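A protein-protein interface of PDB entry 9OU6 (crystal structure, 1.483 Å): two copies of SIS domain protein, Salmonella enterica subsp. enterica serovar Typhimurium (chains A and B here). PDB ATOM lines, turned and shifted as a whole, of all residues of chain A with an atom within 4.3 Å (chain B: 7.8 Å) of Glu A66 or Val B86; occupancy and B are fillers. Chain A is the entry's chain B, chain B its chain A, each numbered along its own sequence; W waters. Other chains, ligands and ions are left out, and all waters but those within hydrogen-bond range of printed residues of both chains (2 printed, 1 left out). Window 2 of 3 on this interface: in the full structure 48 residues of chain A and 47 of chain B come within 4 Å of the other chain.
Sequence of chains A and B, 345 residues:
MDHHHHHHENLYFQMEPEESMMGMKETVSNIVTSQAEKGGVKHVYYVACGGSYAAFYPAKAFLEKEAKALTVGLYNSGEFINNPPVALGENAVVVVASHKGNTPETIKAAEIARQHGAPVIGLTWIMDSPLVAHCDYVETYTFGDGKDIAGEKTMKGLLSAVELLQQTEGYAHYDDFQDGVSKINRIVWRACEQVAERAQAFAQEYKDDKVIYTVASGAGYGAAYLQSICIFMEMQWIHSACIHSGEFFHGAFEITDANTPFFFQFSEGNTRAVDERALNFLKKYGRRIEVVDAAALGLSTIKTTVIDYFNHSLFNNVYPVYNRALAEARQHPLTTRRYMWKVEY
The backbone carbonyl oxygen (O) of Lys A68 lies within hydrogen-bond range of a ring nitrogen (NE2) of His B43, at 3.0 Å.
N of Val B86 is in hydrogen-bond range of O of Lys A65.
The backbone carbonyl oxygen (O) of Pro B84 lies within hydrogen-bond range of the side-chain amino group (NZ) of Lys A65 (2.9 Å).
OD1 of Asn B83 is in hydrogen-bond range of NZ of Lys A65 (2.7 Å).
OE1 of Glu A66 lies within hydrogen-bond range of OH of Tyr A309 (2.7 Å).
Among the printed residues, merely in contact across the chains: Glu A66 with Val B86 (3.3 Å), Glu A64 with Pro B85 (3.5 Å), Lys A65 with Pro B85 (3.7 Å), Ala A67 with Ala B87 (3.8 Å) and Glu A64 with Tyr B75 (3.97 Å).
Leu A63 touches none of the printed residues of chain B.
Glu A66 touches just one residue of chain B: Val B86.
Of chain B, only Ala B87 (3.8 Å) comes within 4 Å of Ala A67.
Tyr A171 touches none of the printed residues of chain B.
Of the printed residues of chain A, Asn B83 touches Lys A65 (2.7 Å).
Of the printed residues of chain A, Pro B84 touches Lys A65.
Val B86 touches just these residues of chain A: Lys A65 (2.9 Å) and Glu A66 (3.3 Å).
Printed residues of chain A within 4 Å of Ala B87: Ala A67.
The nearest residue of chain B that does not touch Glu A66 is Pro B85 (5.7 Å).
The nearest printed residue of chain B that does not touch Glu A64 is Tyr B45 (4.9 Å).
Of the 11 printed residues of chain B, 7 touch a printed residue of chain A.
Printed residues of chain B that touch a printed residue of chain A: His B43, Tyr B75, Asn B83, Pro B84, Pro B85, Val B86 and Ala B87.
Hydrophobic or aromatic side chains of chain B that line the printed part of chain A: His B43, Tyr B75, Pro B85, Val B86 and Ala B87.
Of the 10 printed residues of chain A, 5 touch a printed residue of chain B.
Printed residues of chain A that touch a printed residue of chain B: Glu A64, Lys A65, Glu A66, Ala A67 and Lys A68.
Among the printed residues, 9 pairs touch across the chains.
Among the printed residues, no Asp or Glu carboxylate lies within 4 Å of a Lys or Arg side-chain nitrogen of the other chain.
No position is printed for both chains.
Of the 9 pairs that touch across the chains among the printed residues, none has its exchanged pair printed and touching as well.
Water W1 lies within hydrogen-bond range of the side-chain hydroxyl (OH) of Tyr B45 (2.7 Å) and the backbone carbonyl oxygen (O) of Glu A64 (2.8 Å).
Water W2 bridges OH of Tyr A309 (2.8 Å) and ND2 of Asn B83 (3.0 Å).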
ATOM      1  N   PHE A  62      17.760 -12.271 -16.587  1.00  0.00           N
ATOM      2  CA  PHE A  62      17.783 -12.248 -18.033  1.00  0.00           C
ATOM      3  C   PHE A  62      18.965 -11.424 -18.561  1.00  0.00           C
ATOM      4  O   PHE A  62      19.793 -11.940 -19.318  1.00  0.00           O
ATOM      5  CB  PHE A  62      16.454 -11.684 -18.522  1.00  0.00           C
ATOM      6  CG  PHE A  62      16.428 -11.657 -20.038  1.00  0.00           C
ATOM      7  CD1 PHE A  62      16.008 -12.754 -20.773  1.00  0.00           C
ATOM      8  CD2 PHE A  62      16.880 -10.536 -20.710  1.00  0.00           C
ATOM      9  CE1 PHE A  62      16.054 -12.707 -22.162  1.00  0.00           C
ATOM     10  CE2 PHE A  62      16.917 -10.499 -22.100  1.00  0.00           C
ATOM     11  CZ  PHE A  62      16.489 -11.578 -22.823  1.00  0.00           C
ATOM     12  N   LEU A  63      19.104 -10.167 -18.114  1.00  0.00           N
ATOM     13  CA  LEU A  63      20.179  -9.363 -18.662  1.00  0.00           C
ATOM     14  C   LEU A  63      21.552  -9.855 -18.189  1.00  0.00           C
ATOM     15  O   LEU A  63      22.541  -9.756 -18.944  1.00  0.00           O
ATOM     16  CB  LEU A  63      19.964  -7.852 -18.452  1.00  0.00           C
ATOM     17  CG  LEU A  63      18.781  -7.223 -19.185  1.00  0.00           C
ATOM     18  CD1 LEU A  63      18.509  -5.794 -18.717  1.00  0.00           C
ATOM     19  CD2 LEU A  63      18.994  -7.296 -20.719  1.00  0.00           C
ATOM     20  N   GLU A  64      21.664 -10.379 -16.976  1.00  0.00           N
ATOM     21  CA  GLU A  64      22.942 -10.941 -16.541  1.00  0.00           C
ATOM     22  C   GLU A  64      23.383 -12.111 -17.416  1.00  0.00           C
ATOM     23  O   GLU A  64      24.531 -12.207 -17.804  1.00  0.00           O
ATOM     24  CB  GLU A  64      22.934 -11.426 -15.096  1.00  0.00           C
ATOM     25  CG  GLU A  64      22.811 -10.232 -14.155  1.00  0.00           C
ATOM     26  CD  GLU A  64      23.049 -10.496 -12.686  1.00  0.00           C
ATOM     27  OE1 GLU A  64      22.590 -11.590 -12.247  1.00  0.00           O
ATOM     28  OE2 GLU A  64      23.668  -9.571 -12.024  1.00  0.00           O
ATOM     29  N   LYS A  65      22.449 -12.980 -17.773  1.00  0.00           N
ATOM     30  CA  LYS A  65      22.785 -14.129 -18.600  1.00  0.00           C
ATOM     31  C   LYS A  65      23.034 -13.733 -20.053  1.00  0.00           C
ATOM     32  O   LYS A  65      23.924 -14.304 -20.672  1.00  0.00           O
ATOM     33  CB  LYS A  65      21.663 -15.160 -18.513  1.00  0.00           C
ATOM     34  CG  LYS A  65      21.756 -16.298 -19.546  1.00  0.00           C
ATOM     35  CD  LYS A  65      22.908 -17.231 -19.247  1.00  0.00           C
ATOM     36  CE  LYS A  65      23.059 -18.255 -20.344  1.00  0.00           C
ATOM     37  NZ  LYS A  65      23.663 -19.496 -19.860  1.00  0.00           N
ATOM     38  N   GLU A  66      22.209 -12.851 -20.611  1.00  0.00           N
ATOM     39  CA  GLU A  66      22.087 -12.755 -22.058  1.00  0.00           C
ATOM     40  C   GLU A  66      22.832 -11.583 -22.677  1.00  0.00           C
ATOM     41  O   GLU A  66      23.048 -11.576 -23.907  1.00  0.00           O
ATOM     42  CB  GLU A  66      20.618 -12.610 -22.478  1.00  0.00           C
ATOM     43  CG  GLU A  66      19.708 -13.737 -21.967  1.00  0.00           C
ATOM     44  CD  GLU A  66      19.878 -15.105 -22.598  1.00  0.00           C
ATOM     45  OE1 GLU A  66      19.240 -16.061 -22.059  1.00  0.00           O
ATOM     46  OE2 GLU A  66      20.678 -15.228 -23.573  1.00  0.00           O
ATOM     47  N   ALA A  67      23.191 -10.548 -21.902  1.00  0.00           N
ATOM     48  CA  ALA A  67      23.687  -9.292 -22.454  1.00  0.00           C
ATOM     49  C   ALA A  67      25.210  -9.262 -22.477  1.00  0.00           C
ATOM     50  O   ALA A  67      25.859  -9.749 -21.557  1.00  0.00           O
ATOM     51  CB  ALA A  67      23.206  -8.093 -21.669  1.00  0.00           C
ATOM     52  N   LYS A  68      25.786  -8.679 -23.532  1.00  0.00           N
ATOM     53  CA  LYS A  68      27.229  -8.427 -23.560  1.00  0.00           C
ATOM     54  C   LYS A  68      27.605  -6.946 -23.447  1.00  0.00           C
ATOM     55  O   LYS A  68      28.793  -6.639 -23.284  1.00  0.00           O
ATOM     56  CB  LYS A  68      27.849  -8.970 -24.850  1.00  0.00           C
ATOM     57  CG  LYS A  68      27.759 -10.458 -24.987  1.00  0.00           C
ATOM     58  CD  LYS A  68      28.359 -10.986 -26.286  1.00  0.00           C
ATOM     59  CE  LYS A  68      27.647 -12.213 -26.754  1.00  0.00           C
ATOM     60  NZ  LYS A  68      28.573 -13.209 -27.302  1.00  0.00           N
ATOM     61  N   LEU A 165      17.341  -5.517 -24.893  1.00  0.00           N
ATOM     62  CA  LEU A 165      18.421  -6.289 -25.449  1.00  0.00           C
ATOM     63  C   LEU A 165      18.254  -6.384 -26.971  1.00  0.00           C
ATOM     64  O   LEU A 165      19.218  -6.151 -27.710  1.00  0.00           O
ATOM     65  CB  LEU A 165      18.551  -7.664 -24.806  1.00  0.00           C
ATOM     66  CG  LEU A 165      19.763  -8.472 -25.254  1.00  0.00           C
ATOM     67  CD1 LEU A 165      21.046  -7.767 -24.847  1.00  0.00           C
ATOM     68  CD2 LEU A 165      19.707  -9.863 -24.674  1.00  0.00           C
ATOM     69  N   TYR A 171      19.112 -10.156 -29.728  1.00  0.00           N
ATOM     70  CA  TYR A 171      18.878 -11.268 -28.817  1.00  0.00           C
ATOM     71  C   TYR A 171      18.596 -12.488 -29.683  1.00  0.00           C
ATOM     72  O   TYR A 171      17.570 -12.535 -30.354  1.00  0.00           O
ATOM     73  CB  TYR A 171      17.711 -10.883 -27.894  1.00  0.00           C
ATOM     74  CG  TYR A 171      17.231 -12.019 -26.982  1.00  0.00           C
ATOM     75  CD1 TYR A 171      18.121 -12.948 -26.439  1.00  0.00           C
ATOM     76  CD2 TYR A 171      15.878 -12.169 -26.722  1.00  0.00           C
ATOM     77  CE1 TYR A 171      17.663 -13.959 -25.606  1.00  0.00           C
ATOM     78  CE2 TYR A 171      15.415 -13.201 -25.934  1.00  0.00           C
ATOM     79  CZ  TYR A 171      16.298 -14.103 -25.391  1.00  0.00           C
ATOM     80  OH  TYR A 171      15.825 -15.146 -24.593  1.00  0.00           O
ATOM     81  N   TYR A 309      13.233 -18.263 -17.717  1.00  0.00           N
ATOM     82  CA  TYR A 309      12.603 -16.963 -17.460  1.00  0.00           C
ATOM     83  C   TYR A 309      11.120 -17.097 -17.132  1.00  0.00           C
ATOM     84  O   TYR A 309      10.500 -16.104 -16.825  1.00  0.00           O
ATOM     85  CB  TYR A 309      12.822 -15.994 -18.635  1.00  0.00           C
ATOM     86  CG  TYR A 309      14.317 -15.908 -18.864  1.00  0.00           C
ATOM     87  CD1 TYR A 309      15.158 -15.426 -17.879  1.00  0.00           C
ATOM     88  CD2 TYR A 309      14.883 -16.355 -20.040  1.00  0.00           C
ATOM     89  CE1 TYR A 309      16.521 -15.463 -18.052  1.00  0.00           C
ATOM     90  CE2 TYR A 309      16.250 -16.366 -20.243  1.00  0.00           C
ATOM     91  CZ  TYR A 309      17.071 -15.896 -19.242  1.00  0.00           C
ATOM     92  OH  TYR A 309      18.408 -15.905 -19.518  1.00  0.00           O
ATOM     93  N   HIS B  43      33.930  -6.985 -18.313  1.00  0.00           N
ATOM     94  CA  HIS B  43      33.026  -7.712 -17.417  1.00  0.00           C
ATOM     95  C   HIS B  43      33.825  -8.298 -16.269  1.00  0.00           C
ATOM     96  O   HIS B  43      34.924  -8.863 -16.449  1.00  0.00           O
ATOM     97  CB  HIS B  43      32.299  -8.870 -18.131  1.00  0.00           C
ATOM     98  CG  HIS B  43      31.676  -8.492 -19.441  1.00  0.00           C
ATOM     99  ND1 HIS B  43      32.128  -8.733 -20.731  1.00  0.00           N
ATOM    100  CD2 HIS B  43      30.580  -7.754 -19.572  1.00  0.00           C
ATOM    101  CE1 HIS B  43      31.315  -8.136 -21.587  1.00  0.00           C
ATOM    102  NE2 HIS B  43      30.348  -7.534 -20.891  1.00  0.00           N
ATOM    103  N   TYR B  45      33.311 -10.864 -12.863  1.00  0.00           N
ATOM    104  CA  TYR B  45      32.454 -11.819 -12.156  1.00  0.00           C
ATOM    105  C   TYR B  45      33.124 -12.221 -10.866  1.00  0.00           C
ATOM    106  O   TYR B  45      34.295 -12.607 -10.822  1.00  0.00           O
ATOM    107  CB  TYR B  45      32.153 -13.088 -12.978  1.00  0.00           C
ATOM    108  CG  TYR B  45      31.446 -12.757 -14.280  1.00  0.00           C
ATOM    109  CD1 TYR B  45      30.119 -12.335 -14.244  1.00  0.00           C
ATOM    110  CD2 TYR B  45      32.060 -12.751 -15.521  1.00  0.00           C
ATOM    111  CE1 TYR B  45      29.411 -11.983 -15.373  1.00  0.00           C
ATOM    112  CE2 TYR B  45      31.372 -12.392 -16.662  1.00  0.00           C
ATOM    113  CZ  TYR B  45      30.052 -11.992 -16.594  1.00  0.00           C
ATOM    114  OH  TYR B  45      29.359 -11.619 -17.678  1.00  0.00           O
ATOM    115  N   TYR B  75      27.916 -14.282  -8.332  1.00  0.00           N
ATOM    116  CA  TYR B  75      27.235 -15.556  -8.502  1.00  0.00           C
ATOM    117  C   TYR B  75      27.641 -16.539  -7.423  1.00  0.00           C
ATOM    118  O   TYR B  75      28.806 -16.661  -7.046  1.00  0.00           O
ATOM    119  CB  TYR B  75      27.673 -16.297  -9.759  1.00  0.00           C
ATOM    120  CG  TYR B  75      27.118 -15.740 -11.046  1.00  0.00           C
ATOM    121  CD1 TYR B  75      27.630 -14.598 -11.641  1.00  0.00           C
ATOM    122  CD2 TYR B  75      26.126 -16.430 -11.721  1.00  0.00           C
ATOM    123  CE1 TYR B  75      27.123 -14.126 -12.841  1.00  0.00           C
ATOM    124  CE2 TYR B  75      25.667 -16.014 -12.947  1.00  0.00           C
ATOM    125  CZ  TYR B  75      26.121 -14.828 -13.492  1.00  0.00           C
ATOM    126  OH  TYR B  75      25.586 -14.443 -14.692  1.00  0.00           O
ATOM    127  N   ASN B  83      24.918 -22.274 -15.277  1.00  0.00           N
ATOM    128  CA  ASN B  83      24.281 -21.237 -16.082  1.00  0.00           C
ATOM    129  C   ASN B  83      25.209 -20.045 -16.282  1.00  0.00           C
ATOM    130  O   ASN B  83      24.880 -18.896 -15.928  1.00  0.00           O
ATOM    131  CB  ASN B  83      22.958 -20.782 -15.483  1.00  0.00           C
ATOM    132  CG  ASN B  83      22.124 -20.036 -16.508  1.00  0.00           C
ATOM    133  OD1 ASN B  83      22.207 -20.263 -17.725  1.00  0.00           O
ATOM    134  ND2 ASN B  83      21.313 -19.129 -16.017  1.00  0.00           N
ATOM    135  N   PRO B  84      26.381 -20.256 -16.924  1.00  0.00           N
ATOM    136  CA  PRO B  84      27.319 -19.162 -17.084  1.00  0.00           C
ATOM    137  C   PRO B  84      26.802 -18.083 -18.032  1.00  0.00           C
ATOM    138  O   PRO B  84      26.131 -18.326 -19.032  1.00  0.00           O
ATOM    139  CB  PRO B  84      28.582 -19.847 -17.596  1.00  0.00           C
ATOM    140  CG  PRO B  84      28.044 -21.069 -18.328  1.00  0.00           C
ATOM    141  CD  PRO B  84      26.895 -21.533 -17.472  1.00  0.00           C
ATOM    142  N   PRO B  85      27.160 -16.823 -17.777  1.00  0.00           N
ATOM    143  CA  PRO B  85      26.704 -15.748 -18.627  1.00  0.00           C
ATOM    144  C   PRO B  85      27.333 -15.816 -20.005  1.00  0.00           C
ATOM    145  O   PRO B  85      28.490 -16.247 -20.127  1.00  0.00           O
ATOM    146  CB  PRO B  85      27.131 -14.509 -17.849  1.00  0.00           C
ATOM    147  CG  PRO B  85      28.278 -14.988 -17.044  1.00  0.00           C
ATOM    148  CD  PRO B  85      28.041 -16.406 -16.687  1.00  0.00           C
ATOM    149  N   VAL B  86      26.610 -15.325 -20.999  1.00  0.00           N
ATOM    150  CA  VAL B  86      27.116 -15.344 -22.361  1.00  0.00           C
ATOM    151  C   VAL B  86      28.348 -14.441 -22.502  1.00  0.00           C
ATOM    152  O   VAL B  86      29.151 -14.645 -23.442  1.00  0.00           O
ATOM    153  CB  VAL B  86      26.073 -15.009 -23.443  1.00  0.00           C
ATOM    154  CG1 VAL B  86      24.885 -15.946 -23.340  1.00  0.00           C
ATOM    155  CG2 VAL B  86      25.638 -13.576 -23.459  1.00  0.00           C
ATOM    156  N   ALA B  87      28.497 -13.443 -21.620  1.00  0.00           N
ATOM    157  CA  ALA B  87      29.642 -12.544 -21.732  1.00  0.00           C
ATOM    158  C   ALA B  87      30.926 -13.138 -21.121  1.00  0.00           C
ATOM    159  O   ALA B  87      31.976 -12.474 -21.079  1.00  0.00           O
ATOM    160  CB  ALA B  87      29.318 -11.198 -21.114  1.00  0.00           C
ATOM    161  N   LEU B  88      30.877 -14.377 -20.621  1.00  0.00           N
ATOM    162  CA  LEU B  88      32.052 -15.039 -20.154  1.00  0.00           C
ATOM    163  C   LEU B  88      32.953 -15.337 -21.349  1.00  0.00           C
ATOM    164  O   LEU B  88      32.599 -16.080 -22.257  1.00  0.00           O
ATOM    165  CB  LEU B  88      31.683 -16.308 -19.411  1.00  0.00           C
ATOM    166  CG  LEU B  88      32.849 -17.037 -18.767  1.00  0.00           C
ATOM    167  CD1 LEU B  88      33.627 -16.157 -17.802  1.00  0.00           C
ATOM    168  CD2 LEU B  88      32.401 -18.326 -18.100  1.00  0.00           C
ATOM    169  N   GLY B  89      34.143 -14.759 -21.331  1.00  0.00           N
ATOM    170  CA  GLY B  89      35.057 -14.870 -22.457  1.00  0.00           C
ATOM    171  C   GLY B  89      36.288 -14.011 -22.201  1.00  0.00           C
ATOM    172  O   GLY B  89      36.615 -13.668 -21.060  1.00  0.00           O
ATOM    173  N   HIS B 116      36.958 -20.602 -21.266  1.00  0.00           N
ATOM    174  CA  HIS B 116      36.352 -19.561 -22.069  1.00  0.00           C
ATOM    175  C   HIS B 116      37.324 -18.423 -22.381  1.00  0.00           C
ATOM    176  O   HIS B 116      36.964 -17.461 -23.070  1.00  0.00           O
ATOM    177  CB  HIS B 116      35.130 -19.050 -21.303  1.00  0.00           C
ATOM    178  CG  HIS B 116      33.978 -19.932 -21.546  1.00  0.00           C
ATOM    179  ND1 HIS B 116      33.618 -20.959 -20.708  1.00  0.00           N
ATOM    180  CD2 HIS B 116      33.139 -19.958 -22.580  1.00  0.00           C
ATOM    181  CE1 HIS B 116      32.529 -21.535 -21.199  1.00  0.00           C
ATOM    182  NE2 HIS B 116      32.243 -20.959 -22.347  1.00  0.00           N
HETATM  183  O   HOH W   1      26.831 -10.745 -17.239  1.00  0.00           O
HETATM  184  O   HOH W   2      19.180 -17.965 -17.713  1.00  0.00           O
